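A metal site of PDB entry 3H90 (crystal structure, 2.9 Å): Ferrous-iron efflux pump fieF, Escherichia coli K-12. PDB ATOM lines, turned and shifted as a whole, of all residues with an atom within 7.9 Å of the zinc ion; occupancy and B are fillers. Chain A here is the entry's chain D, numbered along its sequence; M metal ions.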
ATOM      1  N   LEU A  17      15.222  14.345  -0.365  1.00  0.00           N
ATOM      2  CA  LEU A  17      15.351  13.297  -1.363  1.00  0.00           C
ATOM      3  C   LEU A  17      15.589  13.842  -2.769  1.00  0.00           C
ATOM      4  O   LEU A  17      15.460  13.121  -3.759  1.00  0.00           O
ATOM      5  CB  LEU A  17      14.127  12.392  -1.346  1.00  0.00           C
ATOM      6  CG  LEU A  17      14.517  10.919  -1.232  1.00  0.00           C
ATOM      7  CD1 LEU A  17      15.126  10.629   0.142  1.00  0.00           C
ATOM      8  CD2 LEU A  17      13.332  10.025  -1.441  1.00  0.00           C
ATOM      9  N   LYS A  20      19.142  12.688  -2.457  1.00  0.00           N
ATOM     10  CA  LYS A  20      19.232  11.241  -2.483  1.00  0.00           C
ATOM     11  C   LYS A  20      19.028  10.722  -3.899  1.00  0.00           C
ATOM     12  O   LYS A  20      19.430   9.615  -4.225  1.00  0.00           O
ATOM     13  CB  LYS A  20      18.254  10.603  -1.511  1.00  0.00           C
ATOM     14  CG  LYS A  20      18.832   9.388  -0.812  1.00  0.00           C
ATOM     15  CD  LYS A  20      17.810   8.290  -0.646  1.00  0.00           C
ATOM     16  CE  LYS A  20      17.674   7.424  -1.908  1.00  0.00           C
ATOM     17  NZ  LYS A  20      16.785   6.233  -1.726  1.00  0.00           N
ATOM     18  N   ALA A  35      16.212   1.439  -7.487  1.00  0.00           N
ATOM     19  CA  ALA A  35      15.799   2.205  -6.311  1.00  0.00           C
ATOM     20  C   ALA A  35      16.133   3.693  -6.467  1.00  0.00           C
ATOM     21  O   ALA A  35      16.098   4.464  -5.498  1.00  0.00           O
ATOM     22  CB  ALA A  35      16.429   1.643  -5.038  1.00  0.00           C
ATOM     23  N   VAL A  37      14.521   5.267  -9.086  1.00  0.00           N
ATOM     24  CA  VAL A  37      13.217   5.707  -9.541  1.00  0.00           C
ATOM     25  C   VAL A  37      12.344   5.900  -8.309  1.00  0.00           C
ATOM     26  O   VAL A  37      11.510   6.811  -8.270  1.00  0.00           O
ATOM     27  CB  VAL A  37      12.557   4.678 -10.497  1.00  0.00           C
ATOM     28  CG1 VAL A  37      11.333   5.267 -11.166  1.00  0.00           C
ATOM     29  CG2 VAL A  37      13.559   4.223 -11.542  1.00  0.00           C
ATOM     30  N   ASP A  38      12.546   5.056  -7.296  1.00  0.00           N
ATOM     31  CA  ASP A  38      11.860   5.151  -6.006  1.00  0.00           C
ATOM     32  C   ASP A  38      11.918   6.562  -5.437  1.00  0.00           C
ATOM     33  O   ASP A  38      10.906   7.095  -4.982  1.00  0.00           O
ATOM     34  CB  ASP A  38      12.444   4.139  -5.018  1.00  0.00           C
ATOM     35  CG  ASP A  38      11.818   4.235  -3.623  1.00  0.00           C
ATOM     36  OD1 ASP A  38      10.683   4.745  -3.470  1.00  0.00           O
ATOM     37  OD2 ASP A  38      12.466   3.776  -2.656  1.00  0.00           O
ATOM     38  N   SER A  39      13.099   7.162  -5.452  1.00  0.00           N
ATOM     39  CA  SER A  39      13.263   8.511  -4.937  1.00  0.00           C
ATOM     40  C   SER A  39      12.962   9.590  -5.992  1.00  0.00           C
ATOM     41  O   SER A  39      12.749  10.743  -5.647  1.00  0.00           O
ATOM     42  CB  SER A  39      14.653   8.700  -4.327  1.00  0.00           C
ATOM     43  OG  SER A  39      15.645   8.893  -5.303  1.00  0.00           O
ATOM     44  N   LEU A  40      12.953   9.207  -7.271  1.00  0.00           N
ATOM     45  CA  LEU A  40      12.508  10.115  -8.310  1.00  0.00           C
ATOM     46  C   LEU A  40      11.000  10.291  -8.196  1.00  0.00           C
ATOM     47  O   LEU A  40      10.465  11.377  -8.439  1.00  0.00           O
ATOM     48  CB  LEU A  40      12.895   9.606  -9.712  1.00  0.00           C
ATOM     49  CG  LEU A  40      12.416  10.435 -10.918  1.00  0.00           C
ATOM     50  CD1 LEU A  40      12.983  11.849 -10.930  1.00  0.00           C
ATOM     51  CD2 LEU A  40      12.740   9.710 -12.216  1.00  0.00           C
ATOM     52  N   VAL A  41      10.304   9.216  -7.824  1.00  0.00           N
ATOM     53  CA  VAL A  41       8.896   9.294  -7.488  1.00  0.00           C
ATOM     54  C   VAL A  41       8.758  10.261  -6.316  1.00  0.00           C
ATOM     55  O   VAL A  41       8.053  11.257  -6.422  1.00  0.00           O
ATOM     56  CB  VAL A  41       8.285   7.893  -7.167  1.00  0.00           C
ATOM     57  CG1 VAL A  41       6.903   8.033  -6.540  1.00  0.00           C
ATOM     58  CG2 VAL A  41       8.202   7.035  -8.432  1.00  0.00           C
ATOM     59  N   ASP A  42       9.487   9.972  -5.229  1.00  0.00           N
ATOM     60  CA  ASP A  42       9.413  10.735  -3.973  1.00  0.00           C
ATOM     61  C   ASP A  42       9.587  12.235  -4.157  1.00  0.00           C
ATOM     62  O   ASP A  42       8.894  13.009  -3.506  1.00  0.00           O
ATOM     63  CB  ASP A  42      10.439  10.252  -2.958  1.00  0.00           C
ATOM     64  CG  ASP A  42      10.114   8.888  -2.395  1.00  0.00           C
ATOM     65  OD1 ASP A  42       9.279   8.172  -2.966  1.00  0.00           O
ATOM     66  OD2 ASP A  42      10.710   8.515  -1.361  1.00  0.00           O
ATOM     67  N   ILE A  43      10.500  12.626  -5.026  1.00  0.00           N
ATOM     68  CA  ILE A  43      10.704  14.056  -5.293  1.00  0.00           C
ATOM     69  C   ILE A  43       9.426  14.704  -5.836  1.00  0.00           C
ATOM     70  O   ILE A  43       9.012  15.759  -5.350  1.00  0.00           O
ATOM     71  CB  ILE A  43      11.930  14.312  -6.203  1.00  0.00           C
ATOM     72  CG1 ILE A  43      12.431  15.748  -6.028  1.00  0.00           C
ATOM     73  CG2 ILE A  43      11.623  14.047  -7.669  1.00  0.00           C
ATOM     74  CD1 ILE A  43      13.739  15.996  -6.712  1.00  0.00           C
ATOM     75  N   ALA A  45       6.279  13.141  -5.792  1.00  0.00           N
ATOM     76  CA  ALA A  45       5.275  12.806  -4.789  1.00  0.00           C
ATOM     77  C   ALA A  45       5.250  13.796  -3.641  1.00  0.00           C
ATOM     78  O   ALA A  45       4.207  14.405  -3.367  1.00  0.00           O
ATOM     79  CB  ALA A  45       5.503  11.387  -4.264  1.00  0.00           C
ATOM     80  N   SER A  46       6.392  13.985  -2.994  1.00  0.00           N
ATOM     81  CA  SER A  46       6.504  14.853  -1.816  1.00  0.00           C
ATOM     82  C   SER A  46       6.360  16.335  -2.171  1.00  0.00           C
ATOM     83  O   SER A  46       5.896  17.132  -1.351  1.00  0.00           O
ATOM     84  CB  SER A  46       7.814  14.603  -1.057  1.00  0.00           C
ATOM     85  OG  SER A  46       7.769  13.377  -0.347  1.00  0.00           O
ATOM     86  N   THR A 121      17.257   8.966   5.408  1.00  0.00           N
ATOM     87  CA  THR A 121      15.833   8.705   5.558  1.00  0.00           C
ATOM     88  C   THR A 121      15.452   8.557   7.026  1.00  0.00           C
ATOM     89  O   THR A 121      14.417   9.067   7.442  1.00  0.00           O
ATOM     90  CB  THR A 121      15.393   7.480   4.735  1.00  0.00           C
ATOM     91  OG1 THR A 121      15.943   7.588   3.411  1.00  0.00           O
ATOM     92  CG2 THR A 121      13.888   7.408   4.630  1.00  0.00           C
ATOM     93  N   HIS A 146       5.252   6.651   4.229  1.00  0.00           N
ATOM     94  CA  HIS A 146       6.005   6.164   3.076  1.00  0.00           C
ATOM     95  C   HIS A 146       7.479   5.998   3.394  1.00  0.00           C
ATOM     96  O   HIS A 146       8.086   4.996   3.004  1.00  0.00           O
ATOM     97  CB  HIS A 146       5.888   7.079   1.871  1.00  0.00           C
ATOM     98  CG  HIS A 146       6.943   6.802   0.838  1.00  0.00           C
ATOM     99  ND1 HIS A 146       7.061   5.576   0.214  1.00  0.00           N
ATOM    100  CD2 HIS A 146       7.970   7.551   0.380  1.00  0.00           C
ATOM    101  CE1 HIS A 146       8.090   5.605  -0.613  1.00  0.00           C
ATOM    102  NE2 HIS A 146       8.657   6.789  -0.529  1.00  0.00           N
ATOM    103  N   TYR A 147       8.055   6.987   4.076  1.00  0.00           N
ATOM    104  CA  TYR A 147       9.476   7.012   4.383  1.00  0.00           C
ATOM    105  C   TYR A 147       9.844   6.027   5.481  1.00  0.00           C
ATOM    106  O   TYR A 147      10.965   5.540   5.520  1.00  0.00           O
ATOM    107  CB  TYR A 147       9.967   8.426   4.719  1.00  0.00           C
ATOM    108  CG  TYR A 147       9.904   9.364   3.528  1.00  0.00           C
ATOM    109  CD1 TYR A 147       8.971  10.397   3.497  1.00  0.00           C
ATOM    110  CD2 TYR A 147      10.756   9.203   2.440  1.00  0.00           C
ATOM    111  CE1 TYR A 147       8.884  11.261   2.399  1.00  0.00           C
ATOM    112  CE2 TYR A 147      10.686  10.050   1.340  1.00  0.00           C
ATOM    113  CZ  TYR A 147       9.744  11.088   1.329  1.00  0.00           C
ATOM    114  OH  TYR A 147       9.651  11.944   0.251  1.00  0.00           O
ATOM    115  N   SER A 149       8.599   3.191   5.390  1.00  0.00           N
ATOM    116  CA  SER A 149       8.774   2.037   4.502  1.00  0.00           C
ATOM    117  C   SER A 149      10.150   2.026   3.847  1.00  0.00           C
ATOM    118  O   SER A 149      10.838   1.013   3.864  1.00  0.00           O
ATOM    119  CB  SER A 149       7.665   2.002   3.443  1.00  0.00           C
ATOM    120  OG  SER A 149       7.989   1.136   2.373  1.00  0.00           O
ATOM    121  N   ASP A 150      10.540   3.158   3.268  1.00  0.00           N
ATOM    122  CA  ASP A 150      11.877   3.318   2.696  1.00  0.00           C
ATOM    123  C   ASP A 150      12.969   2.986   3.711  1.00  0.00           C
ATOM    124  O   ASP A 150      13.975   2.376   3.363  1.00  0.00           O
ATOM    125  CB  ASP A 150      12.075   4.737   2.163  1.00  0.00           C
ATOM    126  CG  ASP A 150      11.278   5.012   0.915  1.00  0.00           C
ATOM    127  OD1 ASP A 150      10.472   4.152   0.500  1.00  0.00           O
ATOM    128  OD2 ASP A 150      11.465   6.109   0.343  1.00  0.00           O
ATOM    129  N   VAL A 151      12.742   3.375   4.963  1.00  0.00           N
ATOM    130  CA  VAL A 151      13.659   3.096   6.074  1.00  0.00           C
ATOM    131  C   VAL A 151      13.815   1.605   6.350  1.00  0.00           C
ATOM    132  O   VAL A 151      14.812   1.182   6.927  1.00  0.00           O
ATOM    133  CB  VAL A 151      13.239   3.860   7.361  1.00  0.00           C
ATOM    134  CG1 VAL A 151      13.512   3.051   8.628  1.00  0.00           C
ATOM    135  CG2 VAL A 151      13.948   5.193   7.420  1.00  0.00           C
ATOM    136  N   MET A 153      14.900  -0.768   4.708  1.00  0.00           N
ATOM    137  CA  MET A 153      15.791  -1.060   3.591  1.00  0.00           C
ATOM    138  C   MET A 153      16.806  -2.086   4.074  1.00  0.00           C
ATOM    139  O   MET A 153      17.368  -1.950   5.177  1.00  0.00           O
ATOM    140  CB  MET A 153      16.529   0.208   3.191  1.00  0.00           C
ATOM    141  CG  MET A 153      16.715   0.389   1.713  1.00  0.00           C
ATOM    142  SD  MET A 153      17.216   2.081   1.364  1.00  0.00           S
ATOM    143  CE  MET A 153      16.945   2.167  -0.415  1.00  0.00           C
HETATM  144 ZN    ZN M   1      10.807   6.410  -1.350  1.00  0.00          ZN
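OD2 of Asp 150 binds the zinc ion, at 1.8 Å. OD2 of Asp 42 is bound to the zinc ion (2.1 Å). The zinc ion is bound by NE2 of His 146, 2.3 Å away. The zinc ion has three donor atoms within binding distance. Slightly farther from the zinc ion lies OD1 of Asp 38 (2.7 Å). Slightly farther from the zinc ion lies OD1 of Asp 42 (2.8 Å).
O of Asp 42 lies close to OG of Ser 46 (3.4 Å).
The nearest printed residue that does not touch the zinc ion is Leu 17 (4.4 Å).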
